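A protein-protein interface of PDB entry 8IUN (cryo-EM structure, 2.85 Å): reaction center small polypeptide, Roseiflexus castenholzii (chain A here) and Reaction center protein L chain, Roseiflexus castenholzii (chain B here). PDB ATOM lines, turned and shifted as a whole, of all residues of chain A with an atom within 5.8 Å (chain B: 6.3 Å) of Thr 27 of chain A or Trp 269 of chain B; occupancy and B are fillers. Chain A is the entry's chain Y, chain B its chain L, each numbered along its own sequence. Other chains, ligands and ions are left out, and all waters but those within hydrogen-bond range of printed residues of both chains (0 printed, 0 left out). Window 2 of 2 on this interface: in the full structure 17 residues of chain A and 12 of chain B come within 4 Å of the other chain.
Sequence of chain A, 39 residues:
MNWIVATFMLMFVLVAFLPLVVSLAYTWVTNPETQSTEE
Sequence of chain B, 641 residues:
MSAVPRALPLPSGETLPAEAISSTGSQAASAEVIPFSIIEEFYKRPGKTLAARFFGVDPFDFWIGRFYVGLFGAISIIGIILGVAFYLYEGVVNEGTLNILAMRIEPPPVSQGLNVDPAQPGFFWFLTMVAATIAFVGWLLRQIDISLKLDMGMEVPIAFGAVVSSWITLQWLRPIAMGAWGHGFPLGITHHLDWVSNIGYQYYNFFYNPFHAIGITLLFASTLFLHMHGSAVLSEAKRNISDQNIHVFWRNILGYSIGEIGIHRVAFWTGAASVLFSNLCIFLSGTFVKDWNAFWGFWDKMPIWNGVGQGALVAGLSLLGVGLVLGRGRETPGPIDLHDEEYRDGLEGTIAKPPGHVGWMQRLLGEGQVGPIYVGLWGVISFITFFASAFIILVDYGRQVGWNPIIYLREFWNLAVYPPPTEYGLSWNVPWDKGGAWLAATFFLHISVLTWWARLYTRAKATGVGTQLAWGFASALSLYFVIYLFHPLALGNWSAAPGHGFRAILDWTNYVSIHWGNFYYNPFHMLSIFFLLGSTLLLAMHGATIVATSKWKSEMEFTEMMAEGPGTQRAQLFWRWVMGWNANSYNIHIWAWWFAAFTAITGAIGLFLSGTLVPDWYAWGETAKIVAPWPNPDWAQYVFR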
ATOM      1  N   LEU A  20     -12.905   2.868  13.713  1.00  0.00           N
ATOM      2  CA  LEU A  20     -13.844   2.082  14.510  1.00  0.00           C
ATOM      3  C   LEU A  20     -15.267   2.607  14.368  1.00  0.00           C
ATOM      4  O   LEU A  20     -16.225   1.825  14.306  1.00  0.00           O
ATOM      5  CB  LEU A  20     -13.417   2.084  15.975  1.00  0.00           C
ATOM      6  CG  LEU A  20     -14.156   1.128  16.915  1.00  0.00           C
ATOM      7  CD1 LEU A  20     -13.745  -0.310  16.654  1.00  0.00           C
ATOM      8  CD2 LEU A  20     -13.912   1.502  18.361  1.00  0.00           C
ATOM      9  N   VAL A  22     -16.445   4.162  11.731  1.00  0.00           N
ATOM     10  CA  VAL A  22     -16.891   3.753  10.403  1.00  0.00           C
ATOM     11  C   VAL A  22     -17.264   2.276  10.396  1.00  0.00           C
ATOM     12  O   VAL A  22     -18.200   1.867   9.707  1.00  0.00           O
ATOM     13  CB  VAL A  22     -15.817   4.078   9.348  1.00  0.00           C
ATOM     14  CG1 VAL A  22     -16.280   3.648   7.971  1.00  0.00           C
ATOM     15  CG2 VAL A  22     -15.503   5.559   9.356  1.00  0.00           C
ATOM     16  N   SER A  23     -16.541   1.454  11.158  1.00  0.00           N
ATOM     17  CA  SER A  23     -16.890   0.039  11.260  1.00  0.00           C
ATOM     18  C   SER A  23     -18.271  -0.153  11.878  1.00  0.00           C
ATOM     19  O   SER A  23     -19.083  -0.946  11.380  1.00  0.00           O
ATOM     20  CB  SER A  23     -15.829  -0.694  12.075  1.00  0.00           C
ATOM     21  OG  SER A  23     -16.083  -2.082  12.109  1.00  0.00           O
ATOM     22  N   LEU A  24     -18.558   0.571  12.960  1.00  0.00           N
ATOM     23  CA  LEU A  24     -19.876   0.486  13.586  1.00  0.00           C
ATOM     24  C   LEU A  24     -20.977   0.973  12.649  1.00  0.00           C
ATOM     25  O   LEU A  24     -22.045   0.353  12.552  1.00  0.00           O
ATOM     26  CB  LEU A  24     -19.888   1.286  14.885  1.00  0.00           C
ATOM     27  CG  LEU A  24     -19.253   0.641  16.114  1.00  0.00           C
ATOM     28  CD1 LEU A  24     -18.757   1.704  17.061  1.00  0.00           C
ATOM     29  CD2 LEU A  24     -20.258  -0.241  16.812  1.00  0.00           C
ATOM     30  N   ALA A  25     -20.737   2.086  11.951  1.00  0.00           N
ATOM     31  CA  ALA A  25     -21.736   2.614  11.026  1.00  0.00           C
ATOM     32  C   ALA A  25     -21.968   1.670   9.853  1.00  0.00           C
ATOM     33  O   ALA A  25     -23.103   1.503   9.399  1.00  0.00           O
ATOM     34  CB  ALA A  25     -21.312   3.995  10.532  1.00  0.00           C
ATOM     35  N   TYR A  26     -20.902   1.052   9.340  1.00  0.00           N
ATOM     36  CA  TYR A  26     -21.033   0.069   8.271  1.00  0.00           C
ATOM     37  C   TYR A  26     -21.853  -1.129   8.727  1.00  0.00           C
ATOM     38  O   TYR A  26     -22.716  -1.617   7.988  1.00  0.00           O
ATOM     39  CB  TYR A  26     -19.637  -0.362   7.810  1.00  0.00           C
ATOM     40  CG  TYR A  26     -19.598  -1.408   6.718  1.00  0.00           C
ATOM     41  CD1 TYR A  26     -19.560  -1.043   5.382  1.00  0.00           C
ATOM     42  CD2 TYR A  26     -19.571  -2.761   7.023  1.00  0.00           C
ATOM     43  CE1 TYR A  26     -19.519  -1.992   4.385  1.00  0.00           C
ATOM     44  CE2 TYR A  26     -19.530  -3.714   6.032  1.00  0.00           C
ATOM     45  CZ  TYR A  26     -19.505  -3.323   4.715  1.00  0.00           C
ATOM     46  OH  TYR A  26     -19.466  -4.267   3.721  1.00  0.00           O
ATOM     47  N   THR A  27     -21.600  -1.613   9.946  1.00  0.00           N
ATOM     48  CA  THR A  27     -22.377  -2.731  10.468  1.00  0.00           C
ATOM     49  C   THR A  27     -23.849  -2.365  10.606  1.00  0.00           C
ATOM     50  O   THR A  27     -24.729  -3.172  10.291  1.00  0.00           O
ATOM     51  CB  THR A  27     -21.810  -3.181  11.814  1.00  0.00           C
ATOM     52  OG1 THR A  27     -20.473  -3.659  11.631  1.00  0.00           O
ATOM     53  CG2 THR A  27     -22.657  -4.284  12.409  1.00  0.00           C
ATOM     54  N   TRP A  28     -24.138  -1.152  11.081  1.00  0.00           N
ATOM     55  CA  TRP A  28     -25.529  -0.733  11.225  1.00  0.00           C
ATOM     56  C   TRP A  28     -26.218  -0.598   9.871  1.00  0.00           C
ATOM     57  O   TRP A  28     -27.365  -1.023   9.708  1.00  0.00           O
ATOM     58  CB  TRP A  28     -25.600   0.582  11.993  1.00  0.00           C
ATOM     59  CG  TRP A  28     -26.993   1.051  12.261  1.00  0.00           C
ATOM     60  CD1 TRP A  28     -27.721   1.929  11.515  1.00  0.00           C
ATOM     61  CD2 TRP A  28     -27.830   0.666  13.356  1.00  0.00           C
ATOM     62  NE1 TRP A  28     -28.957   2.114  12.076  1.00  0.00           N
ATOM     63  CE2 TRP A  28     -29.049   1.349  13.207  1.00  0.00           C
ATOM     64  CE3 TRP A  28     -27.668  -0.194  14.444  1.00  0.00           C
ATOM     65  CZ2 TRP A  28     -30.097   1.201  14.107  1.00  0.00           C
ATOM     66  CZ3 TRP A  28     -28.705  -0.337  15.331  1.00  0.00           C
ATOM     67  CH2 TRP A  28     -29.904   0.355  15.160  1.00  0.00           C
ATOM     68  N   VAL A  29     -25.537  -0.004   8.891  1.00  0.00           N
ATOM     69  CA  VAL A  29     -26.160   0.263   7.597  1.00  0.00           C
ATOM     70  C   VAL A  29     -26.379  -1.026   6.814  1.00  0.00           C
ATOM     71  O   VAL A  29     -27.409  -1.200   6.154  1.00  0.00           O
ATOM     72  CB  VAL A  29     -25.314   1.276   6.805  1.00  0.00           C
ATOM     73  CG1 VAL A  29     -25.772   1.348   5.369  1.00  0.00           C
ATOM     74  CG2 VAL A  29     -25.404   2.640   7.442  1.00  0.00           C
ATOM     75  N   THR A  30     -25.417  -1.948   6.863  1.00  0.00           N
ATOM     76  CA  THR A  30     -25.472  -3.110   5.985  1.00  0.00           C
ATOM     77  C   THR A  30     -26.345  -4.231   6.541  1.00  0.00           C
ATOM     78  O   THR A  30     -26.540  -5.241   5.860  1.00  0.00           O
ATOM     79  CB  THR A  30     -24.052  -3.612   5.714  1.00  0.00           C
ATOM     80  OG1 THR A  30     -23.171  -2.490   5.629  1.00  0.00           O
ATOM     81  CG2 THR A  30     -23.985  -4.348   4.398  1.00  0.00           C
ATOM     82  N   ASN A  31     -26.895  -4.072   7.746  1.00  0.00           N
ATOM     83  CA  ASN A  31     -27.737  -5.086   8.381  1.00  0.00           C
ATOM     84  C   ASN A  31     -29.072  -4.456   8.760  1.00  0.00           C
ATOM     85  O   ASN A  31     -29.328  -4.189   9.942  1.00  0.00           O
ATOM     86  CB  ASN A  31     -27.063  -5.686   9.613  1.00  0.00           C
ATOM     87  CG  ASN A  31     -25.844  -6.506   9.268  1.00  0.00           C
ATOM     88  OD1 ASN A  31     -24.727  -5.999   9.251  1.00  0.00           O
ATOM     89  ND2 ASN A  31     -26.053  -7.784   8.988  1.00  0.00           N
ATOM     90  N   GLY B 262     -22.105 -11.822  16.636  1.00  0.00           N
ATOM     91  CA  GLY B 262     -22.037 -10.752  17.631  1.00  0.00           C
ATOM     92  C   GLY B 262     -21.009 -10.976  18.694  1.00  0.00           C
ATOM     93  O   GLY B 262     -20.574  -9.998  19.245  1.00  0.00           O
ATOM     94  N   HIS B 264     -17.977 -12.201  18.124  1.00  0.00           N
ATOM     95  CA  HIS B 264     -16.723 -11.829  17.480  1.00  0.00           C
ATOM     96  C   HIS B 264     -16.686 -10.332  17.155  1.00  0.00           C
ATOM     97  O   HIS B 264     -15.627  -9.695  17.275  1.00  0.00           O
ATOM     98  CB  HIS B 264     -16.496 -12.716  16.244  1.00  0.00           C
ATOM     99  CG  HIS B 264     -16.210 -14.165  16.566  1.00  0.00           C
ATOM    100  ND1 HIS B 264     -17.160 -15.155  16.449  1.00  0.00           N
ATOM    101  CD2 HIS B 264     -15.080 -14.786  16.985  1.00  0.00           C
ATOM    102  CE1 HIS B 264     -16.633 -16.319  16.790  1.00  0.00           C
ATOM    103  NE2 HIS B 264     -15.368 -16.127  17.120  1.00  0.00           N
ATOM    104  N   ARG B 265     -17.836  -9.736  16.813  1.00  0.00           N
ATOM    105  CA  ARG B 265     -17.912  -8.282  16.656  1.00  0.00           C
ATOM    106  C   ARG B 265     -17.604  -7.556  17.960  1.00  0.00           C
ATOM    107  O   ARG B 265     -16.868  -6.562  17.974  1.00  0.00           O
ATOM    108  CB  ARG B 265     -19.297  -7.877  16.161  1.00  0.00           C
ATOM    109  CG  ARG B 265     -19.553  -8.073  14.693  1.00  0.00           C
ATOM    110  CD  ARG B 265     -20.995  -7.758  14.376  1.00  0.00           C
ATOM    111  NE  ARG B 265     -21.321  -8.028  12.983  1.00  0.00           N
ATOM    112  CZ  ARG B 265     -22.553  -8.052  12.494  1.00  0.00           C
ATOM    113  NH1 ARG B 265     -23.604  -7.834  13.262  1.00  0.00           N
ATOM    114  NH2 ARG B 265     -22.733  -8.305  11.203  1.00  0.00           N
ATOM    115  N   VAL B 266     -18.191  -8.019  19.064  1.00  0.00           N
ATOM    116  CA  VAL B 266     -17.964  -7.387  20.362  1.00  0.00           C
ATOM    117  C   VAL B 266     -16.501  -7.502  20.763  1.00  0.00           C
ATOM    118  O   VAL B 266     -15.916  -6.561  21.314  1.00  0.00           O
ATOM    119  CB  VAL B 266     -18.901  -8.002  21.419  1.00  0.00           C
ATOM    120  CG1 VAL B 266     -18.497  -7.576  22.811  1.00  0.00           C
ATOM    121  CG2 VAL B 266     -20.330  -7.591  21.154  1.00  0.00           C
ATOM    122  N   ALA B 267     -15.888  -8.657  20.496  1.00  0.00           N
ATOM    123  CA  ALA B 267     -14.463  -8.837  20.751  1.00  0.00           C
ATOM    124  C   ALA B 267     -13.632  -7.794  20.016  1.00  0.00           C
ATOM    125  O   ALA B 267     -12.795  -7.104  20.617  1.00  0.00           O
ATOM    126  CB  ALA B 267     -14.046 -10.240  20.326  1.00  0.00           C
ATOM    127  N   PHE B 268     -13.861  -7.664  18.710  1.00  0.00           N
ATOM    128  CA  PHE B 268     -13.121  -6.698  17.903  1.00  0.00           C
ATOM    129  C   PHE B 268     -13.288  -5.274  18.441  1.00  0.00           C
ATOM    130  O   PHE B 268     -12.297  -4.562  18.690  1.00  0.00           O
ATOM    131  CB  PHE B 268     -13.598  -6.839  16.452  1.00  0.00           C
ATOM    132  CG  PHE B 268     -13.167  -5.739  15.534  1.00  0.00           C
ATOM    133  CD1 PHE B 268     -11.880  -5.250  15.556  1.00  0.00           C
ATOM    134  CD2 PHE B 268     -14.055  -5.229  14.608  1.00  0.00           C
ATOM    135  CE1 PHE B 268     -11.502  -4.247  14.701  1.00  0.00           C
ATOM    136  CE2 PHE B 268     -13.679  -4.232  13.753  1.00  0.00           C
ATOM    137  CZ  PHE B 268     -12.401  -3.740  13.799  1.00  0.00           C
ATOM    138  N   TRP B 269     -14.537  -4.858  18.670  1.00  0.00           N
ATOM    139  CA  TRP B 269     -14.809  -3.482  19.079  1.00  0.00           C
ATOM    140  C   TRP B 269     -14.217  -3.167  20.448  1.00  0.00           C
ATOM    141  O   TRP B 269     -13.619  -2.100  20.642  1.00  0.00           O
ATOM    142  CB  TRP B 269     -16.315  -3.227  19.077  1.00  0.00           C
ATOM    143  CG  TRP B 269     -16.944  -3.224  17.715  1.00  0.00           C
ATOM    144  CD1 TRP B 269     -16.339  -2.920  16.535  1.00  0.00           C
ATOM    145  CD2 TRP B 269     -18.304  -3.544  17.399  1.00  0.00           C
ATOM    146  NE1 TRP B 269     -17.235  -3.029  15.502  1.00  0.00           N
ATOM    147  CE2 TRP B 269     -18.449  -3.412  16.006  1.00  0.00           C
ATOM    148  CE3 TRP B 269     -19.413  -3.929  18.159  1.00  0.00           C
ATOM    149  CZ2 TRP B 269     -19.655  -3.650  15.360  1.00  0.00           C
ATOM    150  CZ3 TRP B 269     -20.606  -4.165  17.512  1.00  0.00           C
ATOM    151  CH2 TRP B 269     -20.718  -4.026  16.130  1.00  0.00           C
ATOM    152  N   THR B 270     -14.389  -4.069  21.419  1.00  0.00           N
ATOM    153  CA  THR B 270     -13.873  -3.826  22.762  1.00  0.00           C
ATOM    154  C   THR B 270     -12.350  -3.762  22.770  1.00  0.00           C
ATOM    155  O   THR B 270     -11.759  -2.869  23.402  1.00  0.00           O
ATOM    156  CB  THR B 270     -14.368  -4.920  23.704  1.00  0.00           C
ATOM    157  OG1 THR B 270     -15.752  -5.172  23.445  1.00  0.00           O
ATOM    158  CG2 THR B 270     -14.211  -4.501  25.146  1.00  0.00           C
ATOM    159  N   GLY B 271     -11.700  -4.693  22.060  1.00  0.00           N
ATOM    160  CA  GLY B 271     -10.252  -4.673  21.998  1.00  0.00           C
ATOM    161  C   GLY B 271      -9.705  -3.380  21.428  1.00  0.00           C
ATOM    162  O   GLY B 271      -8.709  -2.851  21.925  1.00  0.00           O
ATOM    163  N   ALA B 272     -10.340  -2.851  20.379  1.00  0.00           N
ATOM    164  CA  ALA B 272      -9.852  -1.589  19.817  1.00  0.00           C
ATOM    165  C   ALA B 272     -10.110  -0.411  20.758  1.00  0.00           C
ATOM    166  O   ALA B 272      -9.219   0.427  21.001  1.00  0.00           O
ATOM    167  CB  ALA B 272     -10.493  -1.344  18.454  1.00  0.00           C
ATOM    168  N   ALA B 273     -11.330  -0.325  21.300  1.00  0.00           N
ATOM    169  CA  ALA B 273     -11.695   0.831  22.110  1.00  0.00           C
ATOM    170  C   ALA B 273     -10.838   0.941  23.362  1.00  0.00           C
ATOM    171  O   ALA B 273     -10.604   2.056  23.851  1.00  0.00           O
ATOM    172  CB  ALA B 273     -13.172   0.761  22.480  1.00  0.00           C
ATOM    173  N   SER B 274     -10.352  -0.190  23.887  1.00  0.00           N
ATOM    174  CA  SER B 274      -9.561  -0.158  25.117  1.00  0.00           C
ATOM    175  C   SER B 274      -8.371   0.792  25.005  1.00  0.00           C
ATOM    176  O   SER B 274      -8.114   1.588  25.914  1.00  0.00           O
ATOM    177  CB  SER B 274      -9.091  -1.565  25.472  1.00  0.00           C
ATOM    178  OG  SER B 274      -8.296  -2.113  24.441  1.00  0.00           O
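The backbone carbonyl oxygen of Thr 27 of chain A sits close to the side-chain amide oxygen of Asn 31 of chain A (3.0 Å). The side-chain hydroxyl (OG1) of Thr 27 of chain A lies within hydrogen-bond range of the backbone carbonyl oxygen (O) of Ser 23 of chain A (3.1 Å).
Leu 20 of chain A touches Trp 269 of chain B (CD1 to CD1, 3.7 Å). Leu 20 of chain A touches Ala 272 of chain B. Ser 23 of chain A touches Phe 268 of chain B (OG to CE2, 3.6 Å). Trp 269 of chain B touches Ser 23 of chain A (NE1 to OG, 3.7 Å). Leu 24 of chain A touches Trp 269 of chain B. CZ of Arg 265 of chain B touches CG2 of Thr 27 of chain A, at 3.8 Å. Trp 269 of chain B touches Thr 27 of chain A. OD1 of Asn 31 of chain A touches NH2 of Arg 265 of chain B, 3.6 Å away.
Thr 27 of chain A touches just these residues of chain B: Arg 265 and Trp 269. Trp 269 of chain B touches four residues of chain A. Of the printed residues of chain B, Asn 31 of chain A touches Arg 265. Printed residues of chain B within 4 Å of Leu 20 of chain A: Trp 269 and Ala 272. Printed residues of chain A within 4 Å of Ala 272 of chain B: Leu 20 (3.9 Å). Val 266 of chain B touches none of the printed residues of chain A. Thr 30 of chain A touches none of the printed residues of chain B. The nearest printed residue of chain B that does not touch Thr 27 of chain A is Phe 268 of chain B (7.1 Å).
Of the 12 printed residues of chain B, 4 touch a printed residue of chain A. Hydrophobic or aromatic side chains of chain B within 4 Å of the printed part of chain A: Phe 268, Trp 269 and Ala 272. Of the 11 printed residues of chain A, 5 touch a printed residue of chain B. Among the printed residues, 8 pairs touch across the chains.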
